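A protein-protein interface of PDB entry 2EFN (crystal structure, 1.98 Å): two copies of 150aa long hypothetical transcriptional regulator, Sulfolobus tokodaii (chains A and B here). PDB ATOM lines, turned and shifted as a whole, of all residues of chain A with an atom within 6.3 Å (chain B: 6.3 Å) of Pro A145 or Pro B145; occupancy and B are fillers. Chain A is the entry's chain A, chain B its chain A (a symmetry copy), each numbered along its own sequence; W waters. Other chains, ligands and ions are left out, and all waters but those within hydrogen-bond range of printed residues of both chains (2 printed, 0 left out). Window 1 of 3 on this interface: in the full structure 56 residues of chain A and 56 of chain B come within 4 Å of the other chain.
Trp B92 touches its own counterpart, Trp A92.
Trp A92 touches Glu B143, and with the chains exchanged Glu A143 touches Trp B92.
Trp A92 touches Ser B144, and with the chains exchanged Ser A144 touches Trp B92.
Trp A92 touches Pro B145, and with the chains exchanged Pro A145 touches Trp B92.
Positions printed for both chains: 53, 92, 93, 108, 143, 144, 145, 146, 147 and 148.
Of the 14 pairs that touch across the chains among the printed residues, 14 have their exchanged pair printed and touching as well.
Of the 10 printed residues of chain A, 7 touch a printed residue of chain B.
Among the printed residues, 14 pairs touch across the chains.
Among the printed residues, no Asp or Glu carboxylate lies within 4 Å of a Lys or Arg side-chain nitrogen of the other chain.
The backbone carbonyl oxygen (O) of Ser A144 sits close to the side-chain amide oxygen (OD1) of Asn A146, at 3.5 Å.
The side-chain carboxylate (OE1) of Glu B143 lies within salt-bridge range of the guanidinium group (NH2) of Arg B108, at 3.3 Å.
NH2 of Arg A108 is in salt-bridge range of OE1 of Glu A143 (3.3 Å).
The side-chain amide oxygen (OD1) of Asn B146 sits close to the backbone carbonyl oxygen (O) of Ser B144, at 3.5 Å.
Trp B92 touches Trp A92 (CH2 to CH2, 3.9 Å).
CA of Glu B143 touches O of Trp A92, 3.3 Å away.
CA of Pro B145 touches CE3 of Trp A92, 3.6 Å away.
NH1 of Arg A108 touches O of Ile B147 (3.8 Å).
NH1 of Arg A108 touches CG1 of Val B148, at 3.6 Å.
Trp B92 touches Glu A143 (O to CA, 3.3 Å).
Pro A145 touches Trp B92.
CG of Pro B145 touches CG of Pro A145, at 3.4 Å.
O of Ile A147 touches NH1 of Arg B108 (3.8 Å).
Val A148 touches Arg B108 (CG1 to NH1, 3.6 Å).
Pro B145 touches just these residues of chain A: Trp A92 (3.6 Å), Arg A108 (3.2 Å) and Pro A145 (3.4 Å).
Of the printed residues of chain A, Trp B92 touches Trp A92, Glu A143, Ser A144 and Pro A145.
Of the printed residues of chain B, Ile A147 touches Arg B108.
Of the printed residues of chain B, Arg A108 touches Pro B145 (3.2 Å), Ile B147 (3.8 Å) and Val B148 (3.6 Å).
Of the printed residues of chain B, Val A148 touches Arg B108.
Printed residues of chain A within 4 Å of Arg B108: Pro A145 (3.2 Å), Ile A147 (3.8 Å) and Val A148 (3.6 Å).
Tyr A53 touches none of the printed residues of chain B.
The nearest residue of chain B that does not touch Pro A145 is Glu B143 (5.5 Å).
The nearest printed residue of chain B that does not touch Trp A92 is Ile B147 (4.5 Å).
Water W1 bridges NH1 of Arg A108 and O of Ile B147.
Water W2 lies within hydrogen-bond range of NH1 of Arg B108 and O of Ile A147.
The backbone NH (N) of Ser A144 is in hydrogen-bond range of the backbone carbonyl oxygen (O) of Trp B92, 2.8 Å away.
The backbone carbonyl oxygen (O) of Pro B145 lies within hydrogen-bond range of the guanidinium group (NH1) of Arg A108, at 3.2 Å.
N of Ser B144 sits at hydrogen-bond distance from O of Trp A92 (2.8 Å).
The backbone carbonyl oxygen (O) of Pro A145 is in hydrogen-bond range of the guanidinium group (NH1) of Arg B108 (3.2 Å).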
ATOM      1  N   TYR A  53      -5.332   7.410 -26.613  1.00  0.00           N
ATOM      2  CA  TYR A  53      -6.410   8.374 -26.429  1.00  0.00           C
ATOM      3  C   TYR A  53      -5.926   9.699 -26.989  1.00  0.00           C
ATOM      4  O   TYR A  53      -4.999  10.311 -26.461  1.00  0.00           O
ATOM      5  CB  TYR A  53      -6.778   8.557 -24.957  1.00  0.00           C
ATOM      6  CG  TYR A  53      -7.978   9.465 -24.790  1.00  0.00           C
ATOM      7  CD1 TYR A  53      -9.242   9.065 -25.232  1.00  0.00           C
ATOM      8  CD2 TYR A  53      -7.847  10.740 -24.244  1.00  0.00           C
ATOM      9  CE1 TYR A  53     -10.343   9.914 -25.137  1.00  0.00           C
ATOM     10  CE2 TYR A  53      -8.943  11.600 -24.144  1.00  0.00           C
ATOM     11  CZ  TYR A  53     -10.187  11.180 -24.593  1.00  0.00           C
ATOM     12  OH  TYR A  53     -11.275  12.022 -24.499  1.00  0.00           O
ATOM     13  N   TRP A  92     -19.037   8.213 -34.637  1.00  0.00           N
ATOM     14  CA  TRP A  92     -18.375   7.189 -33.844  1.00  0.00           C
ATOM     15  C   TRP A  92     -19.354   6.363 -33.022  1.00  0.00           C
ATOM     16  O   TRP A  92     -19.026   5.262 -32.583  1.00  0.00           O
ATOM     17  CB  TRP A  92     -17.309   7.792 -32.920  1.00  0.00           C
ATOM     18  CG  TRP A  92     -17.805   8.804 -31.929  1.00  0.00           C
ATOM     19  CD1 TRP A  92     -17.766  10.164 -32.057  1.00  0.00           C
ATOM     20  CD2 TRP A  92     -18.363   8.539 -30.632  1.00  0.00           C
ATOM     21  NE1 TRP A  92     -18.256  10.763 -30.916  1.00  0.00           N
ATOM     22  CE2 TRP A  92     -18.628   9.789 -30.027  1.00  0.00           C
ATOM     23  CE3 TRP A  92     -18.660   7.367 -29.921  1.00  0.00           C
ATOM     24  CZ2 TRP A  92     -19.182   9.900 -28.745  1.00  0.00           C
ATOM     25  CZ3 TRP A  92     -19.210   7.477 -28.647  1.00  0.00           C
ATOM     26  CH2 TRP A  92     -19.465   8.739 -28.073  1.00  0.00           C
ATOM     27  N   GLY A  93     -20.561   6.885 -32.827  1.00  0.00           N
ATOM     28  CA  GLY A  93     -21.547   6.149 -32.055  1.00  0.00           C
ATOM     29  C   GLY A  93     -22.932   6.147 -32.670  1.00  0.00           C
ATOM     30  O   GLY A  93     -23.426   7.185 -33.109  1.00  0.00           O
ATOM     31  N   ARG A 108     -18.280  13.809 -34.671  1.00  0.00           N
ATOM     32  CA  ARG A 108     -17.351  14.909 -34.442  1.00  0.00           C
ATOM     33  C   ARG A 108     -16.841  15.438 -35.779  1.00  0.00           C
ATOM     34  O   ARG A 108     -16.501  14.656 -36.666  1.00  0.00           O
ATOM     35  CB  ARG A 108     -16.139  14.438 -33.633  1.00  0.00           C
ATOM     36  CG  ARG A 108     -16.422  13.733 -32.317  1.00  0.00           C
ATOM     37  CD  ARG A 108     -15.102  13.534 -31.586  1.00  0.00           C
ATOM     38  NE  ARG A 108     -15.189  12.701 -30.389  1.00  0.00           N
ATOM     39  CZ  ARG A 108     -14.830  11.420 -30.342  1.00  0.00           C
ATOM     40  NH1 ARG A 108     -14.363  10.817 -31.429  1.00  0.00           N
ATOM     41  NH2 ARG A 108     -14.914  10.747 -29.201  1.00  0.00           N
ATOM     42  N   GLU A 143     -16.096  12.703 -20.760  1.00  0.00           N
ATOM     43  CA  GLU A 143     -16.158  11.753 -21.861  1.00  0.00           C
ATOM     44  C   GLU A 143     -15.034  10.747 -21.697  1.00  0.00           C
ATOM     45  O   GLU A 143     -13.954  10.909 -22.256  1.00  0.00           O
ATOM     46  CB  GLU A 143     -16.037  12.439 -23.222  1.00  0.00           C
ATOM     47  CG  GLU A 143     -16.385  11.484 -24.359  1.00  0.00           C
ATOM     48  CD  GLU A 143     -16.234  12.100 -25.732  1.00  0.00           C
ATOM     49  OE1 GLU A 143     -15.092  12.161 -26.234  1.00  0.00           O
ATOM     50  OE2 GLU A 143     -17.258  12.529 -26.307  1.00  0.00           O
ATOM     51  N   SER A 144     -15.302   9.707 -20.919  1.00  0.00           N
ATOM     52  CA  SER A 144     -14.316   8.669 -20.656  1.00  0.00           C
ATOM     53  C   SER A 144     -14.954   7.299 -20.867  1.00  0.00           C
ATOM     54  O   SER A 144     -15.078   6.507 -19.928  1.00  0.00           O
ATOM     55  CB  SER A 144     -13.815   8.793 -19.217  1.00  0.00           C
ATOM     56  OG  SER A 144     -13.320  10.099 -18.967  1.00  0.00           O
ATOM     57  N   PRO A 145     -15.351   6.996 -22.114  1.00  0.00           N
ATOM     58  CA  PRO A 145     -15.979   5.712 -22.430  1.00  0.00           C
ATOM     59  C   PRO A 145     -15.105   4.516 -22.063  1.00  0.00           C
ATOM     60  O   PRO A 145     -15.602   3.401 -21.910  1.00  0.00           O
ATOM     61  CB  PRO A 145     -16.241   5.818 -23.932  1.00  0.00           C
ATOM     62  CG  PRO A 145     -15.105   6.679 -24.407  1.00  0.00           C
ATOM     63  CD  PRO A 145     -15.049   7.754 -23.344  1.00  0.00           C
ATOM     64  N   ASN A 146     -13.806   4.760 -21.916  1.00  0.00           N
ATOM     65  CA  ASN A 146     -12.851   3.710 -21.564  1.00  0.00           C
ATOM     66  C   ASN A 146     -13.033   3.209 -20.136  1.00  0.00           C
ATOM     67  O   ASN A 146     -12.640   2.086 -19.812  1.00  0.00           O
ATOM     68  CB  ASN A 146     -11.421   4.225 -21.722  1.00  0.00           C
ATOM     69  CG  ASN A 146     -11.173   5.488 -20.927  1.00  0.00           C
ATOM     70  OD1 ASN A 146     -11.834   6.508 -21.145  1.00  0.00           O
ATOM     71  ND2 ASN A 146     -10.224   5.432 -19.998  1.00  0.00           N
ATOM     72  N   ILE A 147     -13.609   4.042 -19.275  1.00  0.00           N
ATOM     73  CA  ILE A 147     -13.820   3.643 -17.889  1.00  0.00           C
ATOM     74  C   ILE A 147     -15.059   2.774 -17.732  1.00  0.00           C
ATOM     75  O   ILE A 147     -16.191   3.266 -17.753  1.00  0.00           O
ATOM     76  CB  ILE A 147     -13.940   4.867 -16.966  1.00  0.00           C
ATOM     77  CG1 ILE A 147     -12.697   5.742 -17.115  1.00  0.00           C
ATOM     78  CG2 ILE A 147     -14.091   4.415 -15.520  1.00  0.00           C
ATOM     79  CD1 ILE A 147     -11.396   4.976 -16.960  1.00  0.00           C
ATOM     80  N   VAL A 148     -14.833   1.474 -17.573  1.00  0.00           N
ATOM     81  CA  VAL A 148     -15.920   0.518 -17.422  1.00  0.00           C
ATOM     82  C   VAL A 148     -15.984  -0.073 -16.018  1.00  0.00           C
ATOM     83  O   VAL A 148     -16.966  -0.718 -15.656  1.00  0.00           O
ATOM     84  CB  VAL A 148     -15.793  -0.630 -18.444  1.00  0.00           C
ATOM     85  CG1 VAL A 148     -15.986  -0.089 -19.855  1.00  0.00           C
ATOM     86  CG2 VAL A 148     -14.439  -1.289 -18.313  1.00  0.00           C
ATOM     87  N   TYR B  53      -9.144  -1.592 -24.486  1.00  0.00           N
ATOM     88  CA  TYR B  53     -10.562  -1.535 -24.819  1.00  0.00           C
ATOM     89  C   TYR B  53     -11.203  -2.796 -24.268  1.00  0.00           C
ATOM     90  O   TYR B  53     -10.922  -3.902 -24.724  1.00  0.00           O
ATOM     91  CB  TYR B  53     -10.801  -1.469 -26.326  1.00  0.00           C
ATOM     92  CG  TYR B  53     -12.269  -1.284 -26.651  1.00  0.00           C
ATOM     93  CD1 TYR B  53     -12.928  -0.097 -26.323  1.00  0.00           C
ATOM     94  CD2 TYR B  53     -13.012  -2.309 -27.234  1.00  0.00           C
ATOM     95  CE1 TYR B  53     -14.292   0.063 -26.564  1.00  0.00           C
ATOM     96  CE2 TYR B  53     -14.379  -2.160 -27.480  1.00  0.00           C
ATOM     97  CZ  TYR B  53     -15.012  -0.972 -27.142  1.00  0.00           C
ATOM     98  OH  TYR B  53     -16.361  -0.816 -27.380  1.00  0.00           O
ATOM     99  N   TRP B  92     -20.217   7.750 -17.931  1.00  0.00           N
ATOM    100  CA  TRP B  92     -18.951   7.985 -18.610  1.00  0.00           C
ATOM    101  C   TRP B  92     -18.984   9.225 -19.491  1.00  0.00           C
ATOM    102  O   TRP B  92     -17.938   9.763 -19.849  1.00  0.00           O
ATOM    103  CB  TRP B  92     -18.526   6.771 -19.445  1.00  0.00           C
ATOM    104  CG  TRP B  92     -19.484   6.354 -20.522  1.00  0.00           C
ATOM    105  CD1 TRP B  92     -20.420   5.361 -20.447  1.00  0.00           C
ATOM    106  CD2 TRP B  92     -19.562   6.880 -21.856  1.00  0.00           C
ATOM    107  NE1 TRP B  92     -21.070   5.229 -21.656  1.00  0.00           N
ATOM    108  CE2 TRP B  92     -20.563   6.148 -22.537  1.00  0.00           C
ATOM    109  CE3 TRP B  92     -18.881   7.894 -22.545  1.00  0.00           C
ATOM    110  CZ2 TRP B  92     -20.903   6.402 -23.871  1.00  0.00           C
ATOM    111  CZ3 TRP B  92     -19.219   8.148 -23.871  1.00  0.00           C
ATOM    112  CH2 TRP B  92     -20.223   7.401 -24.520  1.00  0.00           C
ATOM    113  N   GLY B  93     -20.184   9.688 -19.828  1.00  0.00           N
ATOM    114  CA  GLY B  93     -20.289  10.870 -20.665  1.00  0.00           C
ATOM    115  C   GLY B  93     -21.330  11.866 -20.194  1.00  0.00           C
ATOM    116  O   GLY B  93     -22.449  11.489 -19.850  1.00  0.00           O
ATOM    117  N   ARG B 108     -23.597   3.228 -18.052  1.00  0.00           N
ATOM    118  CA  ARG B 108     -23.685   1.784 -18.231  1.00  0.00           C
ATOM    119  C   ARG B 108     -23.829   1.105 -16.873  1.00  0.00           C
ATOM    120  O   ARG B 108     -23.133   1.462 -15.924  1.00  0.00           O
ATOM    121  CB  ARG B 108     -22.416   1.239 -18.893  1.00  0.00           C
ATOM    122  CG  ARG B 108     -21.991   1.885 -20.201  1.00  0.00           C
ATOM    123  CD  ARG B 108     -20.843   1.074 -20.786  1.00  0.00           C
ATOM    124  NE  ARG B 108     -20.201   1.680 -21.949  1.00  0.00           N
ATOM    125  CZ  ARG B 108     -19.047   2.341 -21.907  1.00  0.00           C
ATOM    126  NH1 ARG B 108     -18.405   2.490 -20.754  1.00  0.00           N
ATOM    127  NH2 ARG B 108     -18.521   2.833 -23.022  1.00  0.00           N
ATOM    128  N   GLU B 143     -19.870   1.913 -31.613  1.00  0.00           N
ATOM    129  CA  GLU B 143     -19.362   2.681 -30.485  1.00  0.00           C
ATOM    130  C   GLU B 143     -17.846   2.606 -30.492  1.00  0.00           C
ATOM    131  O   GLU B 143     -17.251   1.758 -29.835  1.00  0.00           O
ATOM    132  CB  GLU B 143     -19.893   2.163 -29.149  1.00  0.00           C
ATOM    133  CG  GLU B 143     -19.587   3.135 -28.014  1.00  0.00           C
ATOM    134  CD  GLU B 143     -20.050   2.646 -26.659  1.00  0.00           C
ATOM    135  OE1 GLU B 143     -19.335   1.825 -26.048  1.00  0.00           O
ATOM    136  OE2 GLU B 143     -21.132   3.080 -26.209  1.00  0.00           O
ATOM    137  N   SER B 144     -17.230   3.503 -31.250  1.00  0.00           N
ATOM    138  CA  SER B 144     -15.780   3.544 -31.369  1.00  0.00           C
ATOM    139  C   SER B 144     -15.295   4.976 -31.167  1.00  0.00           C
ATOM    140  O   SER B 144     -14.734   5.590 -32.080  1.00  0.00           O
ATOM    141  CB  SER B 144     -15.367   3.045 -32.754  1.00  0.00           C
ATOM    142  OG  SER B 144     -15.904   1.757 -33.006  1.00  0.00           O
ATOM    143  N   PRO B 145     -15.490   5.522 -29.955  1.00  0.00           N
ATOM    144  CA  PRO B 145     -15.069   6.891 -29.651  1.00  0.00           C
ATOM    145  C   PRO B 145     -13.577   7.118 -29.878  1.00  0.00           C
ATOM    146  O   PRO B 145     -13.133   8.255 -30.034  1.00  0.00           O
ATOM    147  CB  PRO B 145     -15.480   7.060 -28.189  1.00  0.00           C
ATOM    148  CG  PRO B 145     -15.326   5.671 -27.637  1.00  0.00           C
ATOM    149  CD  PRO B 145     -15.931   4.821 -28.734  1.00  0.00           C
ATOM    150  N   ASN B 146     -12.813   6.029 -29.903  1.00  0.00           N
ATOM    151  CA  ASN B 146     -11.367   6.097 -30.112  1.00  0.00           C
ATOM    152  C   ASN B 146     -11.002   6.522 -31.530  1.00  0.00           C
ATOM    153  O   ASN B 146      -9.906   7.035 -31.766  1.00  0.00           O
ATOM    154  CB  ASN B 146     -10.732   4.736 -29.832  1.00  0.00           C
ATOM    155  CG  ASN B 146     -11.359   3.628 -30.650  1.00  0.00           C
ATOM    156  OD1 ASN B 146     -12.562   3.371 -30.542  1.00  0.00           O
ATOM    157  ND2 ASN B 146     -10.553   2.966 -31.475  1.00  0.00           N
ATOM    158  N   ILE B 147     -11.905   6.295 -32.479  1.00  0.00           N
ATOM    159  CA  ILE B 147     -11.634   6.669 -33.861  1.00  0.00           C
ATOM    160  C   ILE B 147     -11.888   8.150 -34.106  1.00  0.00           C
ATOM    161  O   ILE B 147     -13.036   8.591 -34.221  1.00  0.00           O
ATOM    162  CB  ILE B 147     -12.481   5.842 -34.841  1.00  0.00           C
ATOM    163  CG1 ILE B 147     -12.229   4.354 -34.604  1.00  0.00           C
ATOM    164  CG2 ILE B 147     -12.126   6.210 -36.275  1.00  0.00           C
ATOM    165  CD1 ILE B 147     -10.757   3.985 -34.594  1.00  0.00           C
ATOM    166  N   VAL B 148     -10.803   8.913 -34.188  1.00  0.00           N
ATOM    167  CA  VAL B 148     -10.889  10.349 -34.408  1.00  0.00           C
ATOM    168  C   VAL B 148     -10.378  10.757 -35.786  1.00  0.00           C
ATOM    169  O   VAL B 148     -10.586  11.889 -36.218  1.00  0.00           O
ATOM    170  CB  VAL B 148     -10.100  11.122 -33.332  1.00  0.00           C
ATOM    171  CG1 VAL B 148     -10.757  10.929 -31.971  1.00  0.00           C
ATOM    172  CG2 VAL B 148      -8.667  10.640 -33.298  1.00  0.00           C
HETATM  173  O   HOH W   1     -14.976  11.093 -34.190  1.00  0.00           O
HETATM  174  O   HOH W   2     -19.311   2.836 -18.083  1.00  0.00           O
